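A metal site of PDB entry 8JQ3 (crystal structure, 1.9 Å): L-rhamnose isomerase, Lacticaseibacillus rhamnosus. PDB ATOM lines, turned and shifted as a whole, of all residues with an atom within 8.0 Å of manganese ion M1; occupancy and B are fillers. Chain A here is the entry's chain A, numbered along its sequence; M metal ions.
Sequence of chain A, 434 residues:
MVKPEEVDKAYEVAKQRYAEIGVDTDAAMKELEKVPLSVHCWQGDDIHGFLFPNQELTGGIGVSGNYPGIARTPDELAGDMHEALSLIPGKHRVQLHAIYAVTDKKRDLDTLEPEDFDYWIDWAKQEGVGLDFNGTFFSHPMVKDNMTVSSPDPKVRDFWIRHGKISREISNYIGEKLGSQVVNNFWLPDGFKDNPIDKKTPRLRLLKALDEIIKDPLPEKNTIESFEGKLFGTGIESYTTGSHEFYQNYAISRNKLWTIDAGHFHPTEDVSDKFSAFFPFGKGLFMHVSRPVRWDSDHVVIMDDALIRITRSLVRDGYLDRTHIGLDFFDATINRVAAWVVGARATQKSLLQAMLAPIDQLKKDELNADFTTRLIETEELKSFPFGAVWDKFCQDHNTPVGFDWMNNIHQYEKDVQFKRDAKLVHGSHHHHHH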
ATOM      1  N   TRP A  42      26.111 -23.743 -15.832  1.00  0.00           N
ATOM      2  CA  TRP A  42      26.259 -22.276 -16.029  1.00  0.00           C
ATOM      3  C   TRP A  42      24.974 -21.630 -16.569  1.00  0.00           C
ATOM      4  O   TRP A  42      24.904 -20.396 -16.539  1.00  0.00           O
ATOM      5  CB  TRP A  42      27.465 -21.911 -16.895  1.00  0.00           C
ATOM      6  CG  TRP A  42      27.601 -22.635 -18.195  1.00  0.00           C
ATOM      7  CD1 TRP A  42      27.155 -22.236 -19.423  1.00  0.00           C
ATOM      8  CD2 TRP A  42      28.310 -23.870 -18.421  1.00  0.00           C
ATOM      9  NE1 TRP A  42      27.504 -23.138 -20.379  1.00  0.00           N
ATOM     10  CE2 TRP A  42      28.221 -24.155 -19.800  1.00  0.00           C
ATOM     11  CE3 TRP A  42      28.999 -24.762 -17.603  1.00  0.00           C
ATOM     12  CZ2 TRP A  42      28.789 -25.291 -20.370  1.00  0.00           C
ATOM     13  CZ3 TRP A  42      29.558 -25.891 -18.165  1.00  0.00           C
ATOM     14  CH2 TRP A  42      29.448 -26.149 -19.530  1.00  0.00           C
ATOM     15  N   GLN A  95      27.933 -30.887 -15.846  1.00  0.00           N
ATOM     16  CA  GLN A  95      29.214 -30.216 -16.207  1.00  0.00           C
ATOM     17  C   GLN A  95      29.435 -29.033 -15.261  1.00  0.00           C
ATOM     18  O   GLN A  95      28.517 -28.193 -15.124  1.00  0.00           O
ATOM     19  CB  GLN A  95      29.195 -29.655 -17.624  1.00  0.00           C
ATOM     20  CG  GLN A  95      28.937 -30.665 -18.728  1.00  0.00           C
ATOM     21  CD  GLN A  95      28.995 -29.984 -20.062  1.00  0.00           C
ATOM     22  OE1 GLN A  95      30.021 -29.423 -20.447  1.00  0.00           O
ATOM     23  NE2 GLN A  95      27.874 -29.981 -20.773  1.00  0.00           N
ATOM     24  N   ASN A 134      35.130 -28.357 -17.052  1.00  0.00           N
ATOM     25  CA  ASN A 134      35.640 -27.375 -18.050  1.00  0.00           C
ATOM     26  C   ASN A 134      36.586 -26.414 -17.324  1.00  0.00           C
ATOM     27  O   ASN A 134      36.163 -25.813 -16.324  1.00  0.00           O
ATOM     28  CB  ASN A 134      34.507 -26.583 -18.722  1.00  0.00           C
ATOM     29  CG  ASN A 134      33.486 -27.429 -19.445  1.00  0.00           C
ATOM     30  OD1 ASN A 134      33.480 -27.505 -20.676  1.00  0.00           O
ATOM     31  ND2 ASN A 134      32.609 -28.067 -18.689  1.00  0.00           N
ATOM     32  N   ASN A 185      36.822 -30.859 -20.503  1.00  0.00           N
ATOM     33  CA  ASN A 185      36.670 -30.215 -21.822  1.00  0.00           C
ATOM     34  C   ASN A 185      37.475 -28.912 -21.845  1.00  0.00           C
ATOM     35  O   ASN A 185      37.304 -28.076 -20.926  1.00  0.00           O
ATOM     36  CB  ASN A 185      35.193 -29.926 -22.151  1.00  0.00           C
ATOM     37  CG  ASN A 185      35.027 -29.393 -23.551  1.00  0.00           C
ATOM     38  OD1 ASN A 185      35.270 -30.115 -24.518  1.00  0.00           O
ATOM     39  ND2 ASN A 185      34.632 -28.143 -23.677  1.00  0.00           N
ATOM     40  N   TRP A 187      37.958 -25.554 -23.963  1.00  0.00           N
ATOM     41  CA  TRP A 187      37.573 -24.533 -24.972  1.00  0.00           C
ATOM     42  C   TRP A 187      38.364 -23.247 -24.706  1.00  0.00           C
ATOM     43  O   TRP A 187      38.371 -22.784 -23.551  1.00  0.00           O
ATOM     44  CB  TRP A 187      36.059 -24.256 -24.994  1.00  0.00           C
ATOM     45  CG  TRP A 187      35.779 -23.165 -25.980  1.00  0.00           C
ATOM     46  CD1 TRP A 187      35.775 -23.274 -27.337  1.00  0.00           C
ATOM     47  CD2 TRP A 187      35.569 -21.771 -25.693  1.00  0.00           C
ATOM     48  NE1 TRP A 187      35.546 -22.054 -27.916  1.00  0.00           N
ATOM     49  CE2 TRP A 187      35.412 -21.110 -26.924  1.00  0.00           C
ATOM     50  CE3 TRP A 187      35.487 -21.027 -24.507  1.00  0.00           C
ATOM     51  CZ2 TRP A 187      35.169 -19.745 -27.012  1.00  0.00           C
ATOM     52  CZ3 TRP A 187      35.253 -19.669 -24.603  1.00  0.00           C
ATOM     53  CH2 TRP A 187      35.099 -19.045 -25.837  1.00  0.00           C
ATOM     54  N   GLU A 228      37.668 -28.679 -27.758  1.00  0.00           N
ATOM     55  CA  GLU A 228      36.463 -28.085 -28.396  1.00  0.00           C
ATOM     56  C   GLU A 228      36.879 -26.944 -29.339  1.00  0.00           C
ATOM     57  O   GLU A 228      37.372 -25.891 -28.852  1.00  0.00           O
ATOM     58  CB  GLU A 228      35.487 -27.582 -27.348  1.00  0.00           C
ATOM     59  CG  GLU A 228      34.266 -26.925 -27.948  1.00  0.00           C
ATOM     60  CD  GLU A 228      33.220 -26.516 -26.938  1.00  0.00           C
ATOM     61  OE1 GLU A 228      33.435 -26.758 -25.734  1.00  0.00           O
ATOM     62  OE2 GLU A 228      32.194 -25.970 -27.351  1.00  0.00           O
ATOM     63  N   GLY A 229      36.662 -27.163 -30.636  1.00  0.00           N
ATOM     64  CA  GLY A 229      36.907 -26.171 -31.683  1.00  0.00           C
ATOM     65  C   GLY A 229      35.700 -25.253 -31.843  1.00  0.00           C
ATOM     66  O   GLY A 229      34.640 -25.549 -31.257  1.00  0.00           O
ATOM     67  N   THR A 259      35.627 -32.707 -29.032  1.00  0.00           N
ATOM     68  CA  THR A 259      34.336 -32.069 -28.683  1.00  0.00           C
ATOM     69  C   THR A 259      33.735 -31.416 -29.929  1.00  0.00           C
ATOM     70  O   THR A 259      34.381 -30.518 -30.505  1.00  0.00           O
ATOM     71  CB  THR A 259      34.486 -31.039 -27.559  1.00  0.00           C
ATOM     72  OG1 THR A 259      34.947 -31.740 -26.404  1.00  0.00           O
ATOM     73  CG2 THR A 259      33.188 -30.313 -27.279  1.00  0.00           C
ATOM     74  N   ILE A 260      32.528 -31.871 -30.301  1.00  0.00           N
ATOM     75  CA  ILE A 260      31.709 -31.312 -31.408  1.00  0.00           C
ATOM     76  C   ILE A 260      30.534 -30.538 -30.804  1.00  0.00           C
ATOM     77  O   ILE A 260      29.626 -31.189 -30.251  1.00  0.00           O
ATOM     78  CB  ILE A 260      31.222 -32.429 -32.342  1.00  0.00           C
ATOM     79  CG1 ILE A 260      32.397 -33.144 -33.020  1.00  0.00           C
ATOM     80  CG2 ILE A 260      30.212 -31.893 -33.355  1.00  0.00           C
ATOM     81  CD1 ILE A 260      32.046 -34.512 -33.549  1.00  0.00           C
ATOM     82  N   ASP A 261      30.558 -29.214 -30.888  1.00  0.00           N
ATOM     83  CA  ASP A 261      29.440 -28.346 -30.441  1.00  0.00           C
ATOM     84  C   ASP A 261      28.610 -27.988 -31.673  1.00  0.00           C
ATOM     85  O   ASP A 261      29.156 -27.395 -32.614  1.00  0.00           O
ATOM     86  CB  ASP A 261      29.925 -27.135 -29.658  1.00  0.00           C
ATOM     87  CG  ASP A 261      28.806 -26.236 -29.167  1.00  0.00           C
ATOM     88  OD1 ASP A 261      27.963 -25.842 -29.999  1.00  0.00           O
ATOM     89  OD2 ASP A 261      28.758 -25.953 -27.949  1.00  0.00           O
ATOM     90  N   ALA A 262      27.331 -28.353 -31.669  1.00  0.00           N
ATOM     91  CA  ALA A 262      26.422 -28.279 -32.840  1.00  0.00           C
ATOM     92  C   ALA A 262      26.195 -26.826 -33.271  1.00  0.00           C
ATOM     93  O   ALA A 262      25.689 -26.619 -34.383  1.00  0.00           O
ATOM     94  CB  ALA A 262      25.136 -28.986 -32.504  1.00  0.00           C
ATOM     95  N   GLY A 263      26.606 -25.859 -32.455  1.00  0.00           N
ATOM     96  CA  GLY A 263      26.425 -24.417 -32.718  1.00  0.00           C
ATOM     97  C   GLY A 263      27.640 -23.765 -33.364  1.00  0.00           C
ATOM     98  O   GLY A 263      27.533 -22.601 -33.762  1.00  0.00           O
ATOM     99  N   HIS A 264      28.765 -24.478 -33.474  1.00  0.00           N
ATOM    100  CA  HIS A 264      30.098 -23.866 -33.717  1.00  0.00           C
ATOM    101  C   HIS A 264      30.606 -24.139 -35.144  1.00  0.00           C
ATOM    102  O   HIS A 264      31.811 -23.932 -35.377  1.00  0.00           O
ATOM    103  CB  HIS A 264      31.076 -24.335 -32.628  1.00  0.00           C
ATOM    104  CG  HIS A 264      30.721 -23.812 -31.271  1.00  0.00           C
ATOM    105  ND1 HIS A 264      31.509 -24.035 -30.160  1.00  0.00           N
ATOM    106  CD2 HIS A 264      29.669 -23.081 -30.845  1.00  0.00           C
ATOM    107  CE1 HIS A 264      30.955 -23.466 -29.110  1.00  0.00           C
ATOM    108  NE2 HIS A 264      29.819 -22.863 -29.510  1.00  0.00           N
ATOM    109  N   PHE A 286      32.882 -35.880 -27.362  1.00  0.00           N
ATOM    110  CA  PHE A 286      31.978 -35.116 -26.473  1.00  0.00           C
ATOM    111  C   PHE A 286      31.048 -34.334 -27.407  1.00  0.00           C
ATOM    112  O   PHE A 286      31.506 -33.365 -28.018  1.00  0.00           O
ATOM    113  CB  PHE A 286      32.788 -34.226 -25.527  1.00  0.00           C
ATOM    114  CG  PHE A 286      32.080 -33.803 -24.274  1.00  0.00           C
ATOM    115  CD1 PHE A 286      30.762 -34.164 -24.028  1.00  0.00           C
ATOM    116  CD2 PHE A 286      32.743 -33.047 -23.321  1.00  0.00           C
ATOM    117  CE1 PHE A 286      30.125 -33.785 -22.854  1.00  0.00           C
ATOM    118  CE2 PHE A 286      32.103 -32.655 -22.150  1.00  0.00           C
ATOM    119  CZ  PHE A 286      30.794 -33.024 -21.922  1.00  0.00           C
ATOM    120  N   MET A 287      29.806 -34.807 -27.573  1.00  0.00           N
ATOM    121  CA  MET A 287      28.797 -34.144 -28.447  1.00  0.00           C
ATOM    122  C   MET A 287      28.029 -33.117 -27.612  1.00  0.00           C
ATOM    123  O   MET A 287      27.255 -33.539 -26.739  1.00  0.00           O
ATOM    124  CB  MET A 287      27.839 -35.174 -29.058  1.00  0.00           C
ATOM    125  CG  MET A 287      26.783 -34.583 -29.962  1.00  0.00           C
ATOM    126  SD  MET A 287      27.417 -33.942 -31.530  1.00  0.00           S
ATOM    127  CE  MET A 287      26.803 -32.257 -31.447  1.00  0.00           C
ATOM    128  N   HIS A 288      28.278 -31.837 -27.868  1.00  0.00           N
ATOM    129  CA  HIS A 288      27.602 -30.683 -27.216  1.00  0.00           C
ATOM    130  C   HIS A 288      26.428 -30.252 -28.095  1.00  0.00           C
ATOM    131  O   HIS A 288      26.665 -29.569 -29.113  1.00  0.00           O
ATOM    132  CB  HIS A 288      28.571 -29.514 -27.019  1.00  0.00           C
ATOM    133  CG  HIS A 288      29.504 -29.676 -25.869  1.00  0.00           C
ATOM    134  ND1 HIS A 288      30.234 -28.608 -25.361  1.00  0.00           N
ATOM    135  CD2 HIS A 288      29.810 -30.746 -25.101  1.00  0.00           C
ATOM    136  CE1 HIS A 288      30.968 -29.036 -24.345  1.00  0.00           C
ATOM    137  NE2 HIS A 288      30.723 -30.331 -24.167  1.00  0.00           N
ATOM    138  N   VAL A 289      25.211 -30.642 -27.725  1.00  0.00           N
ATOM    139  CA  VAL A 289      23.970 -30.187 -28.409  1.00  0.00           C
ATOM    140  C   VAL A 289      23.698 -28.756 -27.970  1.00  0.00           C
ATOM    141  O   VAL A 289      23.727 -28.460 -26.751  1.00  0.00           O
ATOM    142  CB  VAL A 289      22.785 -31.135 -28.172  1.00  0.00           C
ATOM    143  CG1 VAL A 289      22.942 -32.424 -28.962  1.00  0.00           C
ATOM    144  CG2 VAL A 289      22.555 -31.419 -26.691  1.00  0.00           C
ATOM    145  N   SER A 290      23.472 -27.897 -28.958  1.00  0.00           N
ATOM    146  CA  SER A 290      23.282 -26.432 -28.817  1.00  0.00           C
ATOM    147  C   SER A 290      22.583 -25.961 -30.095  1.00  0.00           C
ATOM    148  O   SER A 290      22.878 -26.517 -31.152  1.00  0.00           O
ATOM    149  CB  SER A 290      24.601 -25.731 -28.620  1.00  0.00           C
ATOM    150  OG  SER A 290      24.417 -24.378 -28.273  1.00  0.00           O
ATOM    151  N   ASP A 296      26.605 -18.434 -33.438  1.00  0.00           N
ATOM    152  CA  ASP A 296      26.762 -19.207 -32.175  1.00  0.00           C
ATOM    153  C   ASP A 296      25.966 -18.497 -31.076  1.00  0.00           C
ATOM    154  O   ASP A 296      26.570 -17.851 -30.217  1.00  0.00           O
ATOM    155  CB  ASP A 296      28.237 -19.400 -31.845  1.00  0.00           C
ATOM    156  CG  ASP A 296      28.461 -20.072 -30.505  1.00  0.00           C
ATOM    157  OD1 ASP A 296      27.613 -20.916 -30.126  1.00  0.00           O
ATOM    158  OD2 ASP A 296      29.489 -19.747 -29.854  1.00  0.00           O
ATOM    159  N   ASP A 298      23.700 -19.955 -28.947  1.00  0.00           N
ATOM    160  CA  ASP A 298      23.542 -20.808 -27.738  1.00  0.00           C
ATOM    161  C   ASP A 298      22.068 -20.834 -27.301  1.00  0.00           C
ATOM    162  O   ASP A 298      21.802 -20.752 -26.088  1.00  0.00           O
ATOM    163  CB  ASP A 298      24.457 -20.294 -26.620  1.00  0.00           C
ATOM    164  CG  ASP A 298      25.939 -20.465 -26.936  1.00  0.00           C
ATOM    165  OD1 ASP A 298      26.266 -21.402 -27.683  1.00  0.00           O
ATOM    166  OD2 ASP A 298      26.739 -19.634 -26.469  1.00  0.00           O
ATOM    167  N   GLY A 326      26.576 -33.852 -24.024  1.00  0.00           N
ATOM    168  CA  GLY A 326      26.439 -32.696 -23.115  1.00  0.00           C
ATOM    169  C   GLY A 326      25.460 -31.658 -23.663  1.00  0.00           C
ATOM    170  O   GLY A 326      25.320 -31.560 -24.895  1.00  0.00           O
ATOM    171  N   LEU A 327      24.783 -30.924 -22.775  1.00  0.00           N
ATOM    172  CA  LEU A 327      23.993 -29.722 -23.130  1.00  0.00           C
ATOM    173  C   LEU A 327      24.941 -28.524 -23.052  1.00  0.00           C
ATOM    174  O   LEU A 327      25.760 -28.496 -22.100  1.00  0.00           O
ATOM    175  CB  LEU A 327      22.812 -29.546 -22.173  1.00  0.00           C
ATOM    176  CG  LEU A 327      21.840 -30.715 -22.085  1.00  0.00           C
ATOM    177  CD1 LEU A 327      20.662 -30.351 -21.196  1.00  0.00           C
ATOM    178  CD2 LEU A 327      21.357 -31.140 -23.460  1.00  0.00           C
ATOM    179  N   ASP A 328      24.861 -27.608 -24.022  1.00  0.00           N
ATOM    180  CA  ASP A 328      25.620 -26.328 -23.992  1.00  0.00           C
ATOM    181  C   ASP A 328      24.773 -25.233 -24.645  1.00  0.00           C
ATOM    182  O   ASP A 328      24.723 -25.144 -25.890  1.00  0.00           O
ATOM    183  CB  ASP A 328      27.002 -26.446 -24.641  1.00  0.00           C
ATOM    184  CG  ASP A 328      27.875 -25.249 -24.333  1.00  0.00           C
ATOM    185  OD1 ASP A 328      27.317 -24.201 -23.908  1.00  0.00           O
ATOM    186  OD2 ASP A 328      29.104 -25.355 -24.524  1.00  0.00           O
ATOM    187  N   PHE A 329      24.136 -24.428 -23.820  1.00  0.00           N
ATOM    188  CA  PHE A 329      23.300 -23.298 -24.285  1.00  0.00           C
ATOM    189  C   PHE A 329      23.127 -22.347 -23.103  1.00  0.00           C
ATOM    190  O   PHE A 329      23.428 -22.721 -21.961  1.00  0.00           O
ATOM    191  CB  PHE A 329      21.975 -23.801 -24.879  1.00  0.00           C
ATOM    192  CG  PHE A 329      21.151 -24.722 -24.013  1.00  0.00           C
ATOM    193  CD1 PHE A 329      20.483 -24.252 -22.900  1.00  0.00           C
ATOM    194  CD2 PHE A 329      21.025 -26.063 -24.340  1.00  0.00           C
ATOM    195  CE1 PHE A 329      19.714 -25.101 -22.117  1.00  0.00           C
ATOM    196  CE2 PHE A 329      20.256 -26.913 -23.557  1.00  0.00           C
ATOM    197  CZ  PHE A 329      19.598 -26.425 -22.446  1.00  0.00           C
HETATM  198 MN    MN M   1      30.295 -26.482 -26.324  1.00  0.00          MN
HETATM  199 MN    MN M   2      28.066 -22.041 -28.562  1.00  0.00          MN
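Of the 24 residues printed, 4 come within 4 Å of manganese ion M1. Along chain A the residues within 4 Å of manganese ion M1 span positions 228 to 328.
OE2 of Glu 228 binds manganese ion M1, at 2.2 Å. The side-chain carboxylate (OD2) of Asp 261 binds manganese ion M1, at 2.3 Å. A ring nitrogen (ND1) of His 288 is bound to manganese ion M1 (2.3 Å). Manganese ion M1 is bound by OD2 of Asp 328. Manganese ion M1 has four donor atoms within binding distance.
ND1 of His 264 sits close to OE2 of Glu 228. The side-chain carboxylate (OE1) of Glu 228 sits at hydrogen-bond distance from the side-chain amide nitrogen (ND2) of Asn 185, at 2.8 Å. The side-chain carboxylate of Asp 261 lies within hydrogen-bond range of the backbone NH of Gly 263 (2.8 Å). The backbone carbonyl oxygen (O) of Ile 260 lies within hydrogen-bond range of the backbone NH (N) of His 288, 2.8 Å away. The backbone carbonyl oxygen (O) of His 288 sits at hydrogen-bond distance from the backbone NH (N) of Ala 262, at 2.9 Å. The backbone carbonyl oxygen of Asp 328 sits at hydrogen-bond distance from the side-chain hydroxyl of Ser 290, 2.5 Å away. O of Val 289 is in hydrogen-bond range of N of Asp 328, 3.1 Å away.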
